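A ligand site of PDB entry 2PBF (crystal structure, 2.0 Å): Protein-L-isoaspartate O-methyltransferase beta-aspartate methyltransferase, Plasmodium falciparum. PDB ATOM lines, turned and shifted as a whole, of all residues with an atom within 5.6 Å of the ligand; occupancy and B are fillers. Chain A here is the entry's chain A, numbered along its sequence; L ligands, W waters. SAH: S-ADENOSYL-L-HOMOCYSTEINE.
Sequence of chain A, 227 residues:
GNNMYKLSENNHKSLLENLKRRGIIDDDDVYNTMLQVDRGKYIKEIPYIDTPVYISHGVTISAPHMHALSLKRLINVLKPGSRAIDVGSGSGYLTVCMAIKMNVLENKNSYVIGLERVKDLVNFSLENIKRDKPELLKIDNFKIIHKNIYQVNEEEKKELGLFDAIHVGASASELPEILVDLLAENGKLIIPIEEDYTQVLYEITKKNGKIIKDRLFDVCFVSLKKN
O of Thr 60 lies close to SD of the ligand (3.3 Å). Residues that only touch the ligand: Gly 169 (3.2 Å), Val 118 (3.4 Å), Lys 147 (3.4 Å), Leu 224 (3.4 Å), Gly 90 (3.4 Å), Val 222 (3.5 Å), Ser 223 (3.5 Å), Ser 89 (3.5 Å), Ile 61 (3.6 Å), Val 59 (3.6 Å), Tyr 150 (3.8 Å), Ala 170 (3.9 Å), Leu 121 (3.95 Å) and Leu 115 (3.98 Å).
The side-chain carboxylate (OE2) of Glu 116 lies within hydrogen-bond range of an oxygen (O2') of the ligand, 2.4 Å away. NE2 of His 67 lies within hydrogen-bond range of O of the ligand (2.7 Å). N of Lys 225 is in hydrogen-bond range of N7 of the ligand, at 3.1 Å. O of Lys 225 sits at hydrogen-bond distance from N6 of the ligand, 2.7 Å away. OXT of the ligand is in hydrogen-bond range of N of Ser 91. OG of Ser 91 is in hydrogen-bond range of OXT of the ligand. The side-chain amide oxygen of Asn 148 sits at hydrogen-bond distance from a nitrogen (N6) of the ligand (2.8 Å). The backbone NH of Ser 62 sits at hydrogen-bond distance from an oxygen (O) of the ligand (3.0 Å). The side-chain hydroxyl of Ser 62 sits at hydrogen-bond distance from an oxygen (O) of the ligand (3.5 Å). N of Ile 149 lies within hydrogen-bond range of N1 of the ligand, 3.1 Å away. N of the ligand sits close to O of Gly 88, 3.5 Å away. The backbone NH (N) of Arg 117 is in hydrogen-bond range of a nitrogen (N3) of the ligand (3.3 Å).
Water W1 lies within hydrogen-bond range of a nitrogen (N) of the ligand (2.6 Å), the backbone carbonyl oxygen (O) of Gly 88 (2.7 Å), the side-chain carboxylate (OD1) of Asp 86 (2.7 Å), a ring nitrogen (ND1) of His 167 (3.3 Å) and the backbone NH (N) of Gly 169 (3.4 Å). Water W5 lies within hydrogen-bond range of the backbone carbonyl oxygen of Ser 89 (2.7 Å), the side-chain carboxylate of Asp 86 (2.7 Å), a nitrogen (N) of the ligand (2.9 Å) and the backbone NH of Leu 94 (3.0 Å). Water W2 lies within hydrogen-bond range of a nitrogen (N) of the ligand (2.9 Å) and the side-chain hydroxyl of Ser 62 (2.9 Å). Water W4 lies within hydrogen-bond range of NH2 of Arg 117 and O2' of the ligand. Water W3 lies within hydrogen-bond range of OG of Ser 62 (2.8 Å), O of Thr 60 (3.1 Å) and SD of the ligand (3.4 Å).
N of Val 118 lies within hydrogen-bond range of OE2 of Glu 116, 3.0 Å away. The side-chain carboxylate of Glu 116 is in hydrogen-bond range of the backbone NH of Gly 90, 3.1 Å away. The backbone carbonyl oxygen (O) of Lys 225 lies within hydrogen-bond range of the side-chain amide nitrogen (ND2) of Asn 148 (3.1 Å). The side-chain hydroxyl (OG) of Ser 91 is in hydrogen-bond range of the backbone NH (N) of Tyr 93 (3.1 Å). The backbone NH of Tyr 150 lies within hydrogen-bond range of the side-chain amide oxygen of Asn 148 (2.8 Å). The backbone NH of Gly 88 is in hydrogen-bond range of the backbone carbonyl oxygen of Leu 115 (2.7 Å). O of Lys 147 lies within hydrogen-bond range of N of Arg 117 (3.4 Å). N of Ser 89 is in hydrogen-bond range of O of Leu 115, 3.0 Å away.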
ATOM      1  N   ILE A  55     -31.623 -20.106 -13.197  1.00  0.00           N
ATOM      2  CA  ILE A  55     -31.188 -19.496 -11.943  1.00  0.00           C
ATOM      3  C   ILE A  55     -32.278 -18.578 -11.391  1.00  0.00           C
ATOM      4  O   ILE A  55     -32.877 -18.873 -10.352  1.00  0.00           O
ATOM      5  CB  ILE A  55     -29.846 -18.725 -12.084  1.00  0.00           C
ATOM      6  CG1 ILE A  55     -28.805 -19.561 -12.833  1.00  0.00           C
ATOM      7  CG2 ILE A  55     -29.318 -18.317 -10.712  1.00  0.00           C
ATOM      8  CD1 ILE A  55     -27.602 -18.779 -13.373  1.00  0.00           C
ATOM      9  N   VAL A  59     -32.746 -15.970 -16.476  1.00  0.00           N
ATOM     10  CA  VAL A  59     -31.455 -16.492 -16.920  1.00  0.00           C
ATOM     11  C   VAL A  59     -31.068 -17.881 -16.430  1.00  0.00           C
ATOM     12  O   VAL A  59     -31.394 -18.312 -15.329  1.00  0.00           O
ATOM     13  CB  VAL A  59     -30.272 -15.460 -16.729  1.00  0.00           C
ATOM     14  CG1 VAL A  59     -30.672 -14.051 -17.240  1.00  0.00           C
ATOM     15  CG2 VAL A  59     -29.798 -15.438 -15.266  1.00  0.00           C
ATOM     16  N   THR A  60     -30.358 -18.584 -17.299  1.00  0.00           N
ATOM     17  CA  THR A  60     -29.863 -19.906 -17.030  1.00  0.00           C
ATOM     18  C   THR A  60     -28.333 -19.893 -16.957  1.00  0.00           C
ATOM     19  O   THR A  60     -27.670 -19.033 -17.558  1.00  0.00           O
ATOM     20  CB  THR A  60     -30.331 -20.899 -18.115  1.00  0.00           C
ATOM     21  OG1 THR A  60     -29.883 -20.423 -19.385  1.00  0.00           O
ATOM     22  CG2 THR A  60     -31.873 -21.042 -18.139  1.00  0.00           C
ATOM     23  N   ILE A  61     -27.778 -20.816 -16.184  1.00  0.00           N
ATOM     24  CA  ILE A  61     -26.385 -21.200 -16.359  1.00  0.00           C
ATOM     25  C   ILE A  61     -26.396 -22.000 -17.657  1.00  0.00           C
ATOM     26  O   ILE A  61     -27.287 -22.811 -17.874  1.00  0.00           O
ATOM     27  CB  ILE A  61     -25.878 -22.032 -15.162  1.00  0.00           C
ATOM     28  CG1 ILE A  61     -24.399 -22.458 -15.354  1.00  0.00           C
ATOM     29  CG2 ILE A  61     -26.751 -23.266 -14.962  1.00  0.00           C
ATOM     30  CD1 ILE A  61     -23.779 -23.121 -14.109  1.00  0.00           C
ATOM     31  N   SER A  62     -25.440 -21.748 -18.546  1.00  0.00           N
ATOM     32  CA  SER A  62     -25.415 -22.444 -19.832  1.00  0.00           C
ATOM     33  C   SER A  62     -25.233 -23.972 -19.709  1.00  0.00           C
ATOM     34  O   SER A  62     -24.757 -24.483 -18.684  1.00  0.00           O
ATOM     35  CB  SER A  62     -24.368 -21.834 -20.755  1.00  0.00           C
ATOM     36  OG  SER A  62     -24.571 -20.428 -20.883  1.00  0.00           O
ATOM     37  N   HIS A  67     -20.422 -24.124 -22.387  1.00  0.00           N
ATOM     38  CA  HIS A  67     -19.212 -23.717 -21.680  1.00  0.00           C
ATOM     39  C   HIS A  67     -18.004 -24.383 -22.338  1.00  0.00           C
ATOM     40  O   HIS A  67     -16.965 -23.736 -22.571  1.00  0.00           O
ATOM     41  CB  HIS A  67     -19.227 -24.106 -20.190  1.00  0.00           C
ATOM     42  CG  HIS A  67     -20.214 -23.357 -19.333  1.00  0.00           C
ATOM     43  ND1 HIS A  67     -20.850 -23.942 -18.265  1.00  0.00           N
ATOM     44  CD2 HIS A  67     -20.661 -22.073 -19.384  1.00  0.00           C
ATOM     45  CE1 HIS A  67     -21.662 -23.070 -17.700  1.00  0.00           C
ATOM     46  NE2 HIS A  67     -21.557 -21.912 -18.343  1.00  0.00           N
ATOM     47  N   ASP A  86     -15.354 -11.752 -19.148  1.00  0.00           N
ATOM     48  CA  ASP A  86     -16.522 -12.612 -19.335  1.00  0.00           C
ATOM     49  C   ASP A  86     -17.707 -11.692 -19.246  1.00  0.00           C
ATOM     50  O   ASP A  86     -18.039 -11.165 -18.172  1.00  0.00           O
ATOM     51  CB  ASP A  86     -16.583 -13.684 -18.239  1.00  0.00           C
ATOM     52  CG  ASP A  86     -17.713 -14.659 -18.415  1.00  0.00           C
ATOM     53  OD1 ASP A  86     -18.290 -14.759 -19.510  1.00  0.00           O
ATOM     54  OD2 ASP A  86     -18.030 -15.388 -17.430  1.00  0.00           O
ATOM     55  N   VAL A  87     -18.324 -11.475 -20.406  1.00  0.00           N
ATOM     56  CA  VAL A  87     -19.452 -10.572 -20.491  1.00  0.00           C
ATOM     57  C   VAL A  87     -20.749 -11.353 -20.304  1.00  0.00           C
ATOM     58  O   VAL A  87     -21.122 -12.146 -21.170  1.00  0.00           O
ATOM     59  CB  VAL A  87     -19.492  -9.850 -21.863  1.00  0.00           C
ATOM     60  CG1 VAL A  87     -20.742  -8.918 -21.942  1.00  0.00           C
ATOM     61  CG2 VAL A  87     -18.183  -9.052 -22.110  1.00  0.00           C
ATOM     62  N   GLY A  88     -21.435 -11.132 -19.189  1.00  0.00           N
ATOM     63  CA  GLY A  88     -22.658 -11.852 -18.842  1.00  0.00           C
ATOM     64  C   GLY A  88     -22.241 -13.031 -17.999  1.00  0.00           C
ATOM     65  O   GLY A  88     -22.534 -14.189 -18.320  1.00  0.00           O
ATOM     66  N   SER A  89     -21.547 -12.735 -16.901  1.00  0.00           N
ATOM     67  CA  SER A  89     -20.834 -13.774 -16.186  1.00  0.00           C
ATOM     68  C   SER A  89     -21.791 -14.764 -15.477  1.00  0.00           C
ATOM     69  O   SER A  89     -21.420 -15.903 -15.234  1.00  0.00           O
ATOM     70  CB  SER A  89     -19.769 -13.185 -15.245  1.00  0.00           C
ATOM     71  OG  SER A  89     -20.318 -12.166 -14.408  1.00  0.00           O
ATOM     72  N   GLY A  90     -23.010 -14.302 -15.166  1.00  0.00           N
ATOM     73  CA  GLY A  90     -24.087 -15.185 -14.740  1.00  0.00           C
ATOM     74  C   GLY A  90     -23.810 -15.916 -13.447  1.00  0.00           C
ATOM     75  O   GLY A  90     -23.635 -15.267 -12.409  1.00  0.00           O
ATOM     76  N   SER A  91     -23.753 -17.249 -13.510  1.00  0.00           N
ATOM     77  CA  SER A  91     -23.355 -18.087 -12.384  1.00  0.00           C
ATOM     78  C   SER A  91     -21.885 -17.913 -11.973  1.00  0.00           C
ATOM     79  O   SER A  91     -21.474 -18.377 -10.897  1.00  0.00           O
ATOM     80  CB  SER A  91     -23.577 -19.571 -12.738  1.00  0.00           C
ATOM     81  OG  SER A  91     -22.612 -19.964 -13.692  1.00  0.00           O
ATOM     82  N   GLY A  92     -21.100 -17.243 -12.829  1.00  0.00           N
ATOM     83  CA  GLY A  92     -19.628 -17.099 -12.681  1.00  0.00           C
ATOM     84  C   GLY A  92     -18.857 -18.366 -13.074  1.00  0.00           C
ATOM     85  O   GLY A  92     -17.644 -18.437 -12.912  1.00  0.00           O
ATOM     86  N   TYR A  93     -19.569 -19.355 -13.604  1.00  0.00           N
ATOM     87  CA  TYR A  93     -18.935 -20.656 -13.939  1.00  0.00           C
ATOM     88  C   TYR A  93     -17.738 -20.452 -14.875  1.00  0.00           C
ATOM     89  O   TYR A  93     -16.590 -20.870 -14.591  1.00  0.00           O
ATOM     90  CB  TYR A  93     -19.943 -21.685 -14.538  1.00  0.00           C
ATOM     91  CG  TYR A  93     -19.205 -22.993 -14.769  1.00  0.00           C
ATOM     92  CD1 TYR A  93     -19.052 -23.911 -13.722  1.00  0.00           C
ATOM     93  CD2 TYR A  93     -18.548 -23.262 -15.988  1.00  0.00           C
ATOM     94  CE1 TYR A  93     -18.319 -25.083 -13.879  1.00  0.00           C
ATOM     95  CE2 TYR A  93     -17.813 -24.423 -16.165  1.00  0.00           C
ATOM     96  CZ  TYR A  93     -17.709 -25.338 -15.106  1.00  0.00           C
ATOM     97  OH  TYR A  93     -16.956 -26.497 -15.234  1.00  0.00           O
ATOM     98  N   LEU A  94     -18.000 -19.769 -15.974  1.00  0.00           N
ATOM     99  CA  LEU A  94     -16.979 -19.588 -16.993  1.00  0.00           C
ATOM    100  C   LEU A  94     -15.880 -18.616 -16.559  1.00  0.00           C
ATOM    101  O   LEU A  94     -14.722 -18.766 -16.970  1.00  0.00           O
ATOM    102  CB  LEU A  94     -17.591 -19.193 -18.349  1.00  0.00           C
ATOM    103  CG  LEU A  94     -16.705 -19.595 -19.545  1.00  0.00           C
ATOM    104  CD1 LEU A  94     -16.666 -21.108 -19.813  1.00  0.00           C
ATOM    105  CD2 LEU A  94     -17.233 -18.918 -20.707  1.00  0.00           C
ATOM    106  N   LEU A 115     -18.446  -9.306 -16.007  1.00  0.00           N
ATOM    107  CA  LEU A 115     -19.478  -8.264 -15.950  1.00  0.00           C
ATOM    108  C   LEU A 115     -20.847  -8.902 -15.990  1.00  0.00           C
ATOM    109  O   LEU A 115     -21.125  -9.733 -16.870  1.00  0.00           O
ATOM    110  CB  LEU A 115     -19.342  -7.300 -17.128  1.00  0.00           C
ATOM    111  CG  LEU A 115     -18.545  -6.006 -17.033  1.00  0.00           C
ATOM    112  CD1 LEU A 115     -17.195  -6.124 -16.310  1.00  0.00           C
ATOM    113  CD2 LEU A 115     -18.356  -5.436 -18.437  1.00  0.00           C
ATOM    114  N   GLU A 116     -21.708  -8.497 -15.068  1.00  0.00           N
ATOM    115  CA  GLU A 116     -23.054  -9.021 -14.989  1.00  0.00           C
ATOM    116  C   GLU A 116     -24.069  -7.883 -14.734  1.00  0.00           C
ATOM    117  O   GLU A 116     -23.945  -7.126 -13.763  1.00  0.00           O
ATOM    118  CB  GLU A 116     -23.142 -10.118 -13.918  1.00  0.00           C
ATOM    119  CG  GLU A 116     -24.539 -10.531 -13.580  1.00  0.00           C
ATOM    120  CD  GLU A 116     -25.289 -11.068 -14.792  1.00  0.00           C
ATOM    121  OE1 GLU A 116     -24.690 -11.763 -15.634  1.00  0.00           O
ATOM    122  OE2 GLU A 116     -26.483 -10.780 -14.911  1.00  0.00           O
ATOM    123  N   ARG A 117     -25.070  -7.776 -15.620  1.00  0.00           N
ATOM    124  CA  ARG A 117     -26.036  -6.679 -15.552  1.00  0.00           C
ATOM    125  C   ARG A 117     -26.992  -6.795 -14.382  1.00  0.00           C
ATOM    126  O   ARG A 117     -27.462  -5.765 -13.864  1.00  0.00           O
ATOM    127  CB  ARG A 117     -26.795  -6.518 -16.873  1.00  0.00           C
ATOM    128  CG  ARG A 117     -28.074  -7.322 -17.054  1.00  0.00           C
ATOM    129  CD  ARG A 117     -28.755  -6.977 -18.413  1.00  0.00           C
ATOM    130  NE  ARG A 117     -29.772  -5.934 -18.293  1.00  0.00           N
ATOM    131  CZ  ARG A 117     -30.975  -6.090 -17.696  1.00  0.00           C
ATOM    132  NH1 ARG A 117     -31.811  -5.054 -17.660  1.00  0.00           N
ATOM    133  NH2 ARG A 117     -31.345  -7.258 -17.153  1.00  0.00           N
ATOM    134  N   VAL A 118     -27.246  -8.025 -13.933  1.00  0.00           N
ATOM    135  CA  VAL A 118     -28.222  -8.299 -12.876  1.00  0.00           C
ATOM    136  C   VAL A 118     -27.543  -8.552 -11.546  1.00  0.00           C
ATOM    137  O   VAL A 118     -26.686  -9.449 -11.413  1.00  0.00           O
ATOM    138  CB  VAL A 118     -29.175  -9.485 -13.246  1.00  0.00           C
ATOM    139  CG1 VAL A 118     -30.325  -9.576 -12.272  1.00  0.00           C
ATOM    140  CG2 VAL A 118     -29.697  -9.355 -14.657  1.00  0.00           C
ATOM    141  N   LEU A 121     -27.647 -11.849  -9.764  1.00  0.00           N
ATOM    142  CA  LEU A 121     -26.719 -12.785 -10.380  1.00  0.00           C
ATOM    143  C   LEU A 121     -25.266 -12.501 -10.005  1.00  0.00           C
ATOM    144  O   LEU A 121     -24.510 -13.449  -9.728  1.00  0.00           O
ATOM    145  CB  LEU A 121     -26.940 -12.919 -11.891  1.00  0.00           C
ATOM    146  CG  LEU A 121     -28.176 -13.817 -12.101  1.00  0.00           C
ATOM    147  CD1 LEU A 121     -29.028 -13.322 -13.216  1.00  0.00           C
ATOM    148  CD2 LEU A 121     -27.760 -15.275 -12.293  1.00  0.00           C
ATOM    149  N   LYS A 147     -22.527  -4.676 -13.816  1.00  0.00           N
ATOM    150  CA  LYS A 147     -22.371  -3.763 -14.932  1.00  0.00           C
ATOM    151  C   LYS A 147     -22.997  -4.277 -16.213  1.00  0.00           C
ATOM    152  O   LYS A 147     -22.845  -5.441 -16.579  1.00  0.00           O
ATOM    153  CB  LYS A 147     -20.874  -3.507 -15.192  1.00  0.00           C
ATOM    154  CG  LYS A 147     -20.565  -2.475 -16.296  1.00  0.00           C
ATOM    155  CD  LYS A 147     -20.246  -1.138 -15.643  1.00  0.00           C
ATOM    156  CE  LYS A 147     -20.737   0.033 -16.453  1.00  0.00           C
ATOM    157  NZ  LYS A 147     -20.219   1.297 -15.825  1.00  0.00           N
ATOM    158  N   ASN A 148     -23.675  -3.385 -16.909  1.00  0.00           N
ATOM    159  CA  ASN A 148     -24.132  -3.638 -18.261  1.00  0.00           C
ATOM    160  C   ASN A 148     -23.054  -3.165 -19.230  1.00  0.00           C
ATOM    161  O   ASN A 148     -22.572  -2.037 -19.135  1.00  0.00           O
ATOM    162  CB  ASN A 148     -25.427  -2.874 -18.542  1.00  0.00           C
ATOM    163  CG  ASN A 148     -26.039  -3.233 -19.874  1.00  0.00           C
ATOM    164  OD1 ASN A 148     -25.341  -3.420 -20.885  1.00  0.00           O
ATOM    165  ND2 ASN A 148     -27.356  -3.336 -19.884  1.00  0.00           N
ATOM    166  N   ILE A 149     -22.694  -4.034 -20.173  1.00  0.00           N
ATOM    167  CA  ILE A 149     -21.592  -3.783 -21.102  1.00  0.00           C
ATOM    168  C   ILE A 149     -21.876  -2.550 -21.978  1.00  0.00           C
ATOM    169  O   ILE A 149     -20.946  -1.899 -22.479  1.00  0.00           O
ATOM    170  CB  ILE A 149     -21.303  -5.044 -21.960  1.00  0.00           C
ATOM    171  CG1 ILE A 149     -20.044  -4.860 -22.819  1.00  0.00           C
ATOM    172  CG2 ILE A 149     -22.515  -5.438 -22.828  1.00  0.00           C
ATOM    173  CD1 ILE A 149     -18.761  -4.643 -22.054  1.00  0.00           C
ATOM    174  N   TYR A 150     -23.165  -2.256 -22.155  1.00  0.00           N
ATOM    175  CA  TYR A 150     -23.647  -1.161 -23.013  1.00  0.00           C
ATOM    176  C   TYR A 150     -23.640   0.170 -22.272  1.00  0.00           C
ATOM    177  O   TYR A 150     -23.968   1.217 -22.844  1.00  0.00           O
ATOM    178  CB  TYR A 150     -25.065  -1.467 -23.516  1.00  0.00           C
ATOM    179  CG  TYR A 150     -25.160  -2.498 -24.623  1.00  0.00           C
ATOM    180  CD1 TYR A 150     -24.669  -2.233 -25.891  1.00  0.00           C
ATOM    181  CD2 TYR A 150     -25.788  -3.723 -24.401  1.00  0.00           C
ATOM    182  CE1 TYR A 150     -24.753  -3.175 -26.921  1.00  0.00           C
ATOM    183  CE2 TYR A 150     -25.902  -4.663 -25.408  1.00  0.00           C
ATOM    184  CZ  TYR A 150     -25.393  -4.392 -26.671  1.00  0.00           C
ATOM    185  OH  TYR A 150     -25.514  -5.329 -27.657  1.00  0.00           O
ATOM    186  N   HIS A 167     -15.299 -13.223 -23.758  1.00  0.00           N
ATOM    187  CA  HIS A 167     -16.375 -14.164 -23.901  1.00  0.00           C
ATOM    188  C   HIS A 167     -17.662 -13.438 -23.605  1.00  0.00           C
ATOM    189  O   HIS A 167     -17.753 -12.695 -22.635  1.00  0.00           O
ATOM    190  CB  HIS A 167     -16.188 -15.355 -22.974  1.00  0.00           C
ATOM    191  CG  HIS A 167     -17.360 -16.270 -22.973  1.00  0.00           C
ATOM    192  ND1 HIS A 167     -18.379 -16.170 -22.037  1.00  0.00           N
ATOM    193  CD2 HIS A 167     -17.711 -17.270 -23.810  1.00  0.00           C
ATOM    194  CE1 HIS A 167     -19.301 -17.073 -22.300  1.00  0.00           C
ATOM    195  NE2 HIS A 167     -18.914 -17.763 -23.360  1.00  0.00           N
ATOM    196  N   GLY A 169     -21.616 -14.240 -23.027  1.00  0.00           N
ATOM    197  CA  GLY A 169     -22.490 -15.387 -22.783  1.00  0.00           C
ATOM    198  C   GLY A 169     -23.969 -15.092 -23.026  1.00  0.00           C
ATOM    199  O   GLY A 169     -24.827 -15.778 -22.499  1.00  0.00           O
ATOM    200  N   ALA A 170     -24.233 -14.054 -23.843  1.00  0.00           N
ATOM    201  CA  ALA A 170     -25.569 -13.629 -24.170  1.00  0.00           C
ATOM    202  C   ALA A 170     -25.537 -13.094 -25.595  1.00  0.00           C
ATOM    203  O   ALA A 170     -24.521 -12.588 -26.064  1.00  0.00           O
ATOM    204  CB  ALA A 170     -26.071 -12.559 -23.181  1.00  0.00           C
ATOM    205  N   VAL A 222     -29.405 -16.775 -24.009  1.00  0.00           N
ATOM    206  CA  VAL A 222     -30.215 -15.686 -23.494  1.00  0.00           C
ATOM    207  C   VAL A 222     -29.745 -14.389 -24.197  1.00  0.00           C
ATOM    208  O   VAL A 222     -28.619 -14.317 -24.694  1.00  0.00           O
ATOM    209  CB  VAL A 222     -30.178 -15.552 -21.922  1.00  0.00           C
ATOM    210  CG1 VAL A 222     -29.898 -16.909 -21.216  1.00  0.00           C
ATOM    211  CG2 VAL A 222     -29.149 -14.534 -21.453  1.00  0.00           C
ATOM    212  N   SER A 223     -30.613 -13.382 -24.240  1.00  0.00           N
ATOM    213  CA  SER A 223     -30.319 -12.111 -24.915  1.00  0.00           C
ATOM    214  C   SER A 223     -29.379 -11.152 -24.153  1.00  0.00           C
ATOM    215  O   SER A 223     -29.495 -10.980 -22.928  1.00  0.00           O
ATOM    216  CB  SER A 223     -31.623 -11.394 -25.221  1.00  0.00           C
ATOM    217  OG  SER A 223     -31.374 -10.258 -26.026  1.00  0.00           O
ATOM    218  N   LEU A 224     -28.459 -10.524 -24.889  1.00  0.00           N
ATOM    219  CA  LEU A 224     -27.625  -9.436 -24.335  1.00  0.00           C
ATOM    220  C   LEU A 224     -28.424  -8.132 -24.340  1.00  0.00           C
ATOM    221  O   LEU A 224     -28.495  -7.436 -25.355  1.00  0.00           O
ATOM    222  CB  LEU A 224     -26.322  -9.279 -25.123  1.00  0.00           C
ATOM    223  CG  LEU A 224     -25.249  -8.377 -24.516  1.00  0.00           C
ATOM    224  CD1 LEU A 224     -24.606  -9.036 -23.316  1.00  0.00           C
ATOM    225  CD2 LEU A 224     -24.206  -8.009 -25.578  1.00  0.00           C
ATOM    226  N   LYS A 225     -29.030  -7.823 -23.191  1.00  0.00           N
ATOM    227  CA  LYS A 225     -29.975  -6.718 -23.021  1.00  0.00           C
ATOM    228  C   LYS A 225     -29.309  -5.351 -22.945  1.00  0.00           C
ATOM    229  O   LYS A 225     -28.386  -5.139 -22.147  1.00  0.00           O
ATOM    230  CB  LYS A 225     -30.809  -6.948 -21.754  1.00  0.00           C
ATOM    231  CG  LYS A 225     -31.828  -8.071 -21.827  1.00  0.00           C
ATOM    232  CD  LYS A 225     -32.679  -8.063 -20.566  1.00  0.00           C
ATOM    233  CE  LYS A 225     -33.675  -9.220 -20.492  1.00  0.00           C
ATOM    234  NZ  LYS A 225     -34.724  -9.214 -21.576  1.00  0.00           N
ATOM    235  N   LYS A 226     -29.796  -4.430 -23.760  1.00  0.00           N
ATOM    236  CA  LYS A 226     -29.261  -3.076 -23.857  1.00  0.00           C
ATOM    237  C   LYS A 226     -29.658  -2.146 -22.720  1.00  0.00           C
ATOM    238  O   LYS A 226     -29.010  -1.133 -22.488  1.00  0.00           O
ATOM    239  CB  LYS A 226     -29.644  -2.473 -25.197  1.00  0.00           C
ATOM    240  CG  LYS A 226     -28.788  -2.968 -26.327  1.00  0.00           C
ATOM    241  CD  LYS A 226     -29.315  -2.476 -27.639  1.00  0.00           C
ATOM    242  CE  LYS A 226     -28.352  -2.812 -28.732  1.00  0.00           C
ATOM    243  NZ  LYS A 226     -28.929  -2.378 -30.029  1.00  0.00           N
HETATM  244  N   SAH L   1     -21.752 -17.545 -18.669  1.00  0.00           N
HETATM  245  CA  SAH L   1     -23.051 -17.513 -17.936  1.00  0.00           C
HETATM  246  CB  SAH L   1     -24.160 -17.190 -18.906  1.00  0.00           C
HETATM  247  CG  SAH L   1     -25.374 -16.704 -18.118  1.00  0.00           C
HETATM  248  SD  SAH L   1     -26.737 -16.279 -19.210  1.00  0.00           S
HETATM  249  C   SAH L   1     -23.351 -18.809 -17.178  1.00  0.00           C
HETATM  250  O   SAH L   1     -23.171 -19.885 -17.743  1.00  0.00           O
HETATM  251  OXT SAH L   1     -23.768 -18.788 -15.983  1.00  0.00           O
HETATM  252  C5' SAH L   1     -26.097 -14.673 -19.747  1.00  0.00           C
HETATM  253  C4' SAH L   1     -25.938 -13.616 -18.664  1.00  0.00           C
HETATM  254  O4' SAH L   1     -25.756 -12.389 -19.314  1.00  0.00           O
HETATM  255  C3' SAH L   1     -27.119 -13.412 -17.719  1.00  0.00           C
HETATM  256  O3' SAH L   1     -26.684 -13.637 -16.382  1.00  0.00           O
HETATM  257  C2' SAH L   1     -27.549 -11.970 -17.945  1.00  0.00           C
HETATM  258  O2' SAH L   1     -27.974 -11.344 -16.750  1.00  0.00           O
HETATM  259  C1' SAH L   1     -26.284 -11.354 -18.492  1.00  0.00           C
HETATM  260  N9  SAH L   1     -26.456 -10.170 -19.350  1.00  0.00           N
HETATM  261  C8  SAH L   1     -27.459  -9.971 -20.265  1.00  0.00           C
HETATM  262  N7  SAH L   1     -27.231  -8.783 -20.874  1.00  0.00           N
HETATM  263  C5  SAH L   1     -26.122  -8.210 -20.361  1.00  0.00           C
HETATM  264  C6  SAH L   1     -25.469  -6.995 -20.615  1.00  0.00           C
HETATM  265  N6  SAH L   1     -25.907  -6.116 -21.508  1.00  0.00           N
HETATM  266  N1  SAH L   1     -24.318  -6.708 -19.935  1.00  0.00           N
HETATM  267  C2  SAH L   1     -23.830  -7.587 -18.987  1.00  0.00           C
HETATM  268  N3  SAH L   1     -24.492  -8.758 -18.756  1.00  0.00           N
HETATM  269  C4  SAH L   1     -25.622  -9.084 -19.423  1.00  0.00           C
HETATM  270  O   HOH W   1     -20.866 -15.502 -19.933  1.00  0.00           O
HETATM  271  O   HOH W   2     -21.920 -19.225 -20.974  1.00  0.00           O
HETATM  272  O   HOH W   3     -27.082 -19.340 -20.545  1.00  0.00           O
HETATM  273  O   HOH W   4     -30.305  -9.867 -17.974  1.00  0.00           O
HETATM  274  O   HOH W   5     -19.697 -17.406 -16.690  1.00  0.00           O
